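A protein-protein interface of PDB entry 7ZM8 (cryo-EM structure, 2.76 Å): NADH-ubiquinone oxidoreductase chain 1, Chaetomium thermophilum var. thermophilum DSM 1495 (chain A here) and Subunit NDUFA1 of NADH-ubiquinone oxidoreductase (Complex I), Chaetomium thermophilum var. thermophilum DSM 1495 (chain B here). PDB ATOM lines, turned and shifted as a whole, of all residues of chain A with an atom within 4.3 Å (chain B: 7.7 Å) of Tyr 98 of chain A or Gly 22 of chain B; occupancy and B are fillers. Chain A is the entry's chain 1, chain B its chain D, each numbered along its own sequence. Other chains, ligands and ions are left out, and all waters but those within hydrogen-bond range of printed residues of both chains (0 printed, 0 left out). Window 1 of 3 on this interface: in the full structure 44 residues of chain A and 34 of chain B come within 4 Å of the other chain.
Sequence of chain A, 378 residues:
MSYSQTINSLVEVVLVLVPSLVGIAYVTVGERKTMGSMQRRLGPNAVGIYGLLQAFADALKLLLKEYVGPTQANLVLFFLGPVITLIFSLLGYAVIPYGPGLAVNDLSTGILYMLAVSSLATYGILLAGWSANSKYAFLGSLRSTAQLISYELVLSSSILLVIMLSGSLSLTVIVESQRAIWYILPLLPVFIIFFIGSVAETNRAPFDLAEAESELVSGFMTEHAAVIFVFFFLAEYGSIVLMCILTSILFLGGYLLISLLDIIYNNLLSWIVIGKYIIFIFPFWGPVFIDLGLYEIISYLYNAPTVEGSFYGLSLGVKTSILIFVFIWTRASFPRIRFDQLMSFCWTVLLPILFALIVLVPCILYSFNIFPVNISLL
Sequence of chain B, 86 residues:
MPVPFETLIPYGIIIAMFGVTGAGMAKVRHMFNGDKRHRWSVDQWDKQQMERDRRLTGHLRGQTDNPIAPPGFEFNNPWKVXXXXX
The backbone carbonyl oxygen (O) of Val 16 of chain A is in hydrogen-bond range of the side-chain hydroxyl (OG) of Ser 20 of chain A. The side-chain hydroxyl (OG1) of Thr 21 of chain B is in hydrogen-bond range of the backbone carbonyl oxygen (O) of Met 17 of chain B, 3.3 Å away.
Among the printed residues, merely in contact across the chains: Val 16 of chain A with Thr 21 of chain B (3.7 Å), Val 16 of chain A with Met 25 of chain B (3.3 Å), Tyr 98 of chain A with Thr 21 of chain B (3.7 Å), Tyr 98 of chain A with Gly 22 of chain B (3.8 Å), Leu 102 of chain A with Met 25 of chain B (3.7 Å), Leu 102 of chain A with Ala 26 of chain B (3.7 Å), Gly 309 of chain A with Gly 22 of chain B (3.4 Å), Gly 309 of chain A with Ala 23 of chain B (3.7 Å), Ser 310 of chain A with Gly 19 of chain B (3.7 Å), Ser 310 of chain A with Ala 23 of chain B (3.6 Å), Gly 313 of chain A with Phe 18 of chain B (3.4 Å) and Gly 313 of chain A with Gly 19 of chain B (3.9 Å).
Of the printed residues of chain B, Val 16 of chain A touches Thr 21 (3.7 Å) and Met 25 (3.3 Å). Pro 97 of chain A touches none of the printed residues of chain B. Of the printed residues of chain B, Tyr 98 of chain A touches Thr 21 (3.7 Å) and Gly 22 (3.8 Å). Of the printed residues of chain B, Gly 309 of chain A touches Gly 22 (3.4 Å) and Ala 23 (3.7 Å). Printed residues of chain B within 4 Å of Gly 313 of chain A: Phe 18 (3.4 Å) and Gly 19 (3.9 Å). Of the printed residues of chain A, Gly 19 of chain B touches Ser 310 and Gly 313. Gly 22 of chain B touches just these residues of chain A: Tyr 98 and Gly 309. Of the printed residues of chain A, Met 25 of chain B touches Val 16 (3.3 Å) and Leu 102 (3.7 Å). The nearest residue of chain B that does not touch Tyr 98 of chain A is Phe 18 of chain B (4.2 Å). The nearest residue of chain A that does not touch Gly 22 of chain B is Ser 310 of chain A (4.2 Å). The nearest printed residue of chain B that does not touch Val 16 of chain A is Met 17 of chain B (6.9 Å).
Of the 12 printed residues of chain A, 6 touch a printed residue of chain B. Printed residues of chain A that touch a printed residue of chain B: Val 16, Tyr 98, Leu 102, Gly 309, Ser 310 and Gly 313. Hydrophobic or aromatic side chains of chain A within 4 Å of the printed part of chain B: Val 16, Tyr 98 and Leu 102. Among the printed residues, 12 pairs touch across the chains.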
ATOM      1  N   VAL A  16      -9.830   3.881  15.136  1.00  0.00           N
ATOM      2  CA  VAL A  16      -9.272   5.108  14.514  1.00  0.00           C
ATOM      3  C   VAL A  16      -9.220   6.178  15.584  1.00  0.00           C
ATOM      4  O   VAL A  16      -8.153   6.767  15.767  1.00  0.00           O
ATOM      5  CB  VAL A  16     -10.136   5.590  13.331  1.00  0.00           C
ATOM      6  CG1 VAL A  16      -9.942   7.068  13.034  1.00  0.00           C
ATOM      7  CG2 VAL A  16      -9.894   4.771  12.087  1.00  0.00           C
ATOM      8  N   SER A  20      -5.815   7.644  17.767  1.00  0.00           N
ATOM      9  CA  SER A  20      -5.555   9.040  17.344  1.00  0.00           C
ATOM     10  C   SER A  20      -5.556   9.963  18.559  1.00  0.00           C
ATOM     11  O   SER A  20      -4.735  10.875  18.581  1.00  0.00           O
ATOM     12  CB  SER A  20      -6.522   9.491  16.292  1.00  0.00           C
ATOM     13  OG  SER A  20      -6.245   8.866  15.050  1.00  0.00           O
ATOM     14  N   ILE A  96      -9.682   9.955   6.720  1.00  0.00           N
ATOM     15  CA  ILE A  96      -8.237   9.589   6.622  1.00  0.00           C
ATOM     16  C   ILE A  96      -8.057   8.106   6.260  1.00  0.00           C
ATOM     17  O   ILE A  96      -8.502   7.265   7.049  1.00  0.00           O
ATOM     18  CB  ILE A  96      -7.422  10.008   7.859  1.00  0.00           C
ATOM     19  CG1 ILE A  96      -7.531  11.512   8.128  1.00  0.00           C
ATOM     20  CG2 ILE A  96      -5.977   9.559   7.730  1.00  0.00           C
ATOM     21  CD1 ILE A  96      -7.233  12.380   6.929  1.00  0.00           C
ATOM     22  N   PRO A  97      -7.447   7.738   5.098  1.00  0.00           N
ATOM     23  CA  PRO A  97      -7.198   6.350   4.794  1.00  0.00           C
ATOM     24  C   PRO A  97      -5.891   5.796   5.370  1.00  0.00           C
ATOM     25  O   PRO A  97      -4.859   6.350   5.117  1.00  0.00           O
ATOM     26  CB  PRO A  97      -7.224   6.382   3.265  1.00  0.00           C
ATOM     27  CG  PRO A  97      -6.700   7.742   2.872  1.00  0.00           C
ATOM     28  CD  PRO A  97      -7.032   8.652   4.031  1.00  0.00           C
ATOM     29  N   TYR A  98      -5.980   4.695   6.109  1.00  0.00           N
ATOM     30  CA  TYR A  98      -4.796   4.048   6.724  1.00  0.00           C
ATOM     31  C   TYR A  98      -4.437   2.881   5.820  1.00  0.00           C
ATOM     32  O   TYR A  98      -3.845   1.894   6.288  1.00  0.00           O
ATOM     33  CB  TYR A  98      -5.105   3.664   8.170  1.00  0.00           C
ATOM     34  CG  TYR A  98      -5.584   4.823   9.009  1.00  0.00           C
ATOM     35  CD1 TYR A  98      -6.934   5.116   9.110  1.00  0.00           C
ATOM     36  CD2 TYR A  98      -4.695   5.639   9.683  1.00  0.00           C
ATOM     37  CE1 TYR A  98      -7.389   6.183   9.860  1.00  0.00           C
ATOM     38  CE2 TYR A  98      -5.135   6.709  10.443  1.00  0.00           C
ATOM     39  CZ  TYR A  98      -6.487   6.982  10.534  1.00  0.00           C
ATOM     40  OH  TYR A  98      -6.948   8.029  11.282  1.00  0.00           O
ATOM     41  N   GLY A  99      -4.804   3.004   4.551  1.00  0.00           N
ATOM     42  CA  GLY A  99      -4.635   1.908   3.598  1.00  0.00           C
ATOM     43  C   GLY A  99      -5.566   2.198   2.442  1.00  0.00           C
ATOM     44  O   GLY A  99      -6.323   3.158   2.585  1.00  0.00           O
ATOM     45  N   LEU A 102      -9.172   2.311   3.368  1.00  0.00           N
ATOM     46  CA  LEU A 102      -9.324   1.983   4.808  1.00  0.00           C
ATOM     47  C   LEU A 102      -9.549   3.263   5.582  1.00  0.00           C
ATOM     48  O   LEU A 102      -8.613   3.719   6.237  1.00  0.00           O
ATOM     49  CB  LEU A 102      -8.117   1.199   5.322  1.00  0.00           C
ATOM     50  CG  LEU A 102      -8.049  -0.243   4.831  1.00  0.00           C
ATOM     51  CD1 LEU A 102      -6.638  -0.788   4.926  1.00  0.00           C
ATOM     52  CD2 LEU A 102      -9.031  -1.115   5.592  1.00  0.00           C
ATOM     53  N   GLY A 309      -1.460  -4.014   6.288  1.00  0.00           N
ATOM     54  CA  GLY A 309      -2.108  -2.856   6.874  1.00  0.00           C
ATOM     55  C   GLY A 309      -1.232  -2.160   7.894  1.00  0.00           C
ATOM     56  O   GLY A 309      -1.215  -0.931   7.975  1.00  0.00           O
ATOM     57  N   SER A 310      -0.451  -2.942   8.642  1.00  0.00           N
ATOM     58  CA  SER A 310       0.444  -2.356   9.676  1.00  0.00           C
ATOM     59  C   SER A 310       1.545  -1.517   9.025  1.00  0.00           C
ATOM     60  O   SER A 310       1.807  -0.428   9.538  1.00  0.00           O
ATOM     61  CB  SER A 310       1.027  -3.412  10.563  1.00  0.00           C
ATOM     62  OG  SER A 310       2.134  -4.042   9.939  1.00  0.00           O
ATOM     63  N   TYR A 312       1.388   0.022   6.181  1.00  0.00           N
ATOM     64  CA  TYR A 312       0.796   1.179   5.467  1.00  0.00           C
ATOM     65  C   TYR A 312       0.533   2.256   6.518  1.00  0.00           C
ATOM     66  O   TYR A 312       0.754   3.446   6.230  1.00  0.00           O
ATOM     67  CB  TYR A 312      -0.482   0.768   4.729  1.00  0.00           C
ATOM     68  CG  TYR A 312      -0.308   0.229   3.333  1.00  0.00           C
ATOM     69  CD1 TYR A 312       0.778   0.585   2.553  1.00  0.00           C
ATOM     70  CD2 TYR A 312      -1.253  -0.615   2.774  1.00  0.00           C
ATOM     71  CE1 TYR A 312       0.933   0.104   1.263  1.00  0.00           C
ATOM     72  CE2 TYR A 312      -1.114  -1.109   1.487  1.00  0.00           C
ATOM     73  CZ  TYR A 312      -0.016  -0.746   0.728  1.00  0.00           C
ATOM     74  OH  TYR A 312       0.132  -1.226  -0.542  1.00  0.00           O
ATOM     75  N   GLY A 313       0.078   1.852   7.703  1.00  0.00           N
ATOM     76  CA  GLY A 313      -0.081   2.807   8.811  1.00  0.00           C
ATOM     77  C   GLY A 313       1.242   3.347   9.298  1.00  0.00           C
ATOM     78  O   GLY A 313       1.293   4.529   9.626  1.00  0.00           O
ATOM     79  N   LEU A 316       2.446   6.003   6.890  1.00  0.00           N
ATOM     80  CA  LEU A 316       1.713   7.271   7.098  1.00  0.00           C
ATOM     81  C   LEU A 316       2.084   7.816   8.478  1.00  0.00           C
ATOM     82  O   LEU A 316       2.096   9.040   8.629  1.00  0.00           O
ATOM     83  CB  LEU A 316       0.211   7.006   6.956  1.00  0.00           C
ATOM     84  CG  LEU A 316      -0.716   8.186   7.245  1.00  0.00           C
ATOM     85  CD1 LEU A 316      -0.671   9.201   6.115  1.00  0.00           C
ATOM     86  CD2 LEU A 316      -2.138   7.703   7.468  1.00  0.00           C
ATOM     87  N   ALA B  16       3.631   4.082  16.212  1.00  0.00           N
ATOM     88  CA  ALA B  16       3.010   2.825  16.607  1.00  0.00           C
ATOM     89  C   ALA B  16       1.492   2.938  16.625  1.00  0.00           C
ATOM     90  O   ALA B  16       0.790   1.985  16.269  1.00  0.00           O
ATOM     91  CB  ALA B  16       3.535   2.391  17.972  1.00  0.00           C
ATOM     92  N   MET B  17       0.957   4.093  17.005  1.00  0.00           N
ATOM     93  CA  MET B  17      -0.516   4.301  17.001  1.00  0.00           C
ATOM     94  C   MET B  17      -1.063   4.229  15.574  1.00  0.00           C
ATOM     95  O   MET B  17      -2.065   3.548  15.360  1.00  0.00           O
ATOM     96  CB  MET B  17      -0.921   5.598  17.710  1.00  0.00           C
ATOM     97  CG  MET B  17      -0.775   5.506  19.206  1.00  0.00           C
ATOM     98  SD  MET B  17      -1.399   3.921  19.816  1.00  0.00           S
ATOM     99  CE  MET B  17      -0.449   3.756  21.326  1.00  0.00           C
ATOM    100  N   PHE B  18      -0.439   4.947  14.644  1.00  0.00           N
ATOM    101  CA  PHE B  18      -0.875   4.941  13.225  1.00  0.00           C
ATOM    102  C   PHE B  18      -0.741   3.518  12.694  1.00  0.00           C
ATOM    103  O   PHE B  18      -1.598   3.099  11.899  1.00  0.00           O
ATOM    104  CB  PHE B  18      -0.013   5.907  12.413  1.00  0.00           C
ATOM    105  CG  PHE B  18      -0.449   7.346  12.393  1.00  0.00           C
ATOM    106  CD1 PHE B  18      -0.033   8.230  13.373  1.00  0.00           C
ATOM    107  CD2 PHE B  18      -1.244   7.827  11.371  1.00  0.00           C
ATOM    108  CE1 PHE B  18      -0.423   9.558  13.346  1.00  0.00           C
ATOM    109  CE2 PHE B  18      -1.632   9.157  11.343  1.00  0.00           C
ATOM    110  CZ  PHE B  18      -1.223  10.017  12.332  1.00  0.00           C
ATOM    111  N   GLY B  19       0.325   2.823  13.099  1.00  0.00           N
ATOM    112  CA  GLY B  19       0.496   1.411  12.721  1.00  0.00           C
ATOM    113  C   GLY B  19      -0.631   0.524  13.207  1.00  0.00           C
ATOM    114  O   GLY B  19      -1.070  -0.300  12.415  1.00  0.00           O
ATOM    115  N   VAL B  20      -1.107   0.691  14.445  1.00  0.00           N
ATOM    116  CA  VAL B  20      -2.111  -0.221  14.985  1.00  0.00           C
ATOM    117  C   VAL B  20      -3.494   0.116  14.450  1.00  0.00           C
ATOM    118  O   VAL B  20      -4.361  -0.759  14.359  1.00  0.00           O
ATOM    119  CB  VAL B  20      -2.079  -0.226  16.528  1.00  0.00           C
ATOM    120  CG1 VAL B  20      -2.481   1.116  17.089  1.00  0.00           C
ATOM    121  CG2 VAL B  20      -2.961  -1.327  17.084  1.00  0.00           C
ATOM    122  N   THR B  21      -3.738   1.376  14.092  1.00  0.00           N
ATOM    123  CA  THR B  21      -4.981   1.700  13.406  1.00  0.00           C
ATOM    124  C   THR B  21      -5.049   0.997  12.062  1.00  0.00           C
ATOM    125  O   THR B  21      -6.008   0.279  11.770  1.00  0.00           O
ATOM    126  CB  THR B  21      -5.118   3.210  13.221  1.00  0.00           C
ATOM    127  OG1 THR B  21      -5.186   3.842  14.500  1.00  0.00           O
ATOM    128  CG2 THR B  21      -6.378   3.537  12.434  1.00  0.00           C
ATOM    129  N   GLY B  22      -4.015   1.170  11.240  1.00  0.00           N
ATOM    130  CA  GLY B  22      -4.004   0.537   9.936  1.00  0.00           C
ATOM    131  C   GLY B  22      -3.909  -0.971  10.025  1.00  0.00           C
ATOM    132  O   GLY B  22      -4.460  -1.685   9.186  1.00  0.00           O
ATOM    133  N   ALA B  23      -3.201  -1.476  11.033  1.00  0.00           N
ATOM    134  CA  ALA B  23      -3.094  -2.918  11.208  1.00  0.00           C
ATOM    135  C   ALA B  23      -4.444  -3.538  11.529  1.00  0.00           C
ATOM    136  O   ALA B  23      -4.880  -4.484  10.864  1.00  0.00           O
ATOM    137  CB  ALA B  23      -2.090  -3.239  12.310  1.00  0.00           C
ATOM    138  N   GLY B  24      -5.194  -2.930  12.443  1.00  0.00           N
ATOM    139  CA  GLY B  24      -6.455  -3.530  12.906  1.00  0.00           C
ATOM    140  C   GLY B  24      -7.628  -3.254  12.012  1.00  0.00           C
ATOM    141  O   GLY B  24      -8.537  -4.077  11.979  1.00  0.00           O
ATOM    142  N   MET B  25      -7.640  -2.104  11.356  1.00  0.00           N
ATOM    143  CA  MET B  25      -8.733  -1.733  10.422  1.00  0.00           C
ATOM    144  C   MET B  25      -8.747  -2.650   9.201  1.00  0.00           C
ATOM    145  O   MET B  25      -9.839  -2.960   8.728  1.00  0.00           O
ATOM    146  CB  MET B  25      -8.611  -0.268  10.006  1.00  0.00           C
ATOM    147  CG  MET B  25      -9.951   0.405   9.877  1.00  0.00           C
ATOM    148  SD  MET B  25      -9.837   2.184  10.100  1.00  0.00           S
ATOM    149  CE  MET B  25     -11.412   2.697   9.421  1.00  0.00           C
ATOM    150  N   ALA B  26      -7.579  -3.026   8.692  1.00  0.00           N
ATOM    151  CA  ALA B  26      -7.478  -3.917   7.520  1.00  0.00           C
ATOM    152  C   ALA B  26      -7.856  -5.339   7.922  1.00  0.00           C
ATOM    153  O   ALA B  26      -8.210  -6.127   7.034  1.00  0.00           O
ATOM    154  CB  ALA B  26      -6.074  -3.866   6.986  1.00  0.00           C
ATOM    155  N   LYS B  27      -7.794  -5.647   9.208  1.00  0.00           N
ATOM    156  CA  LYS B  27      -8.025  -7.034   9.659  1.00  0.00           C
ATOM    157  C   LYS B  27      -9.523  -7.237   9.791  1.00  0.00           C
ATOM    158  O   LYS B  27     -10.042  -8.182   9.209  1.00  0.00           O
ATOM    159  CB  LYS B  27      -7.310  -7.315  10.982  1.00  0.00           C
ATOM    160  CG  LYS B  27      -7.554  -8.704  11.555  1.00  0.00           C
ATOM    161  CD  LYS B  27      -7.298  -9.812  10.559  1.00  0.00           C
ATOM    162  CE  LYS B  27      -7.778 -11.162  11.044  1.00  0.00           C
ATOM    163  NZ  LYS B  27      -7.797 -12.159   9.949  1.00  0.00           N
ATOM    164  N   VAL B  28     -10.202  -6.259  10.359  1.00  0.00           N
ATOM    165  CA  VAL B  28     -11.670  -6.346  10.585  1.00  0.00           C
ATOM    166  C   VAL B  28     -12.433  -6.171   9.270  1.00  0.00           C
ATOM    167  O   VAL B  28     -13.502  -6.759   9.162  1.00  0.00           O
ATOM    168  CB  VAL B  28     -12.111  -5.356  11.676  1.00  0.00           C
ATOM    169  CG1 VAL B  28     -11.545  -5.748  13.027  1.00  0.00           C
ATOM    170  CG2 VAL B  28     -11.758  -3.920  11.337  1.00  0.00           C
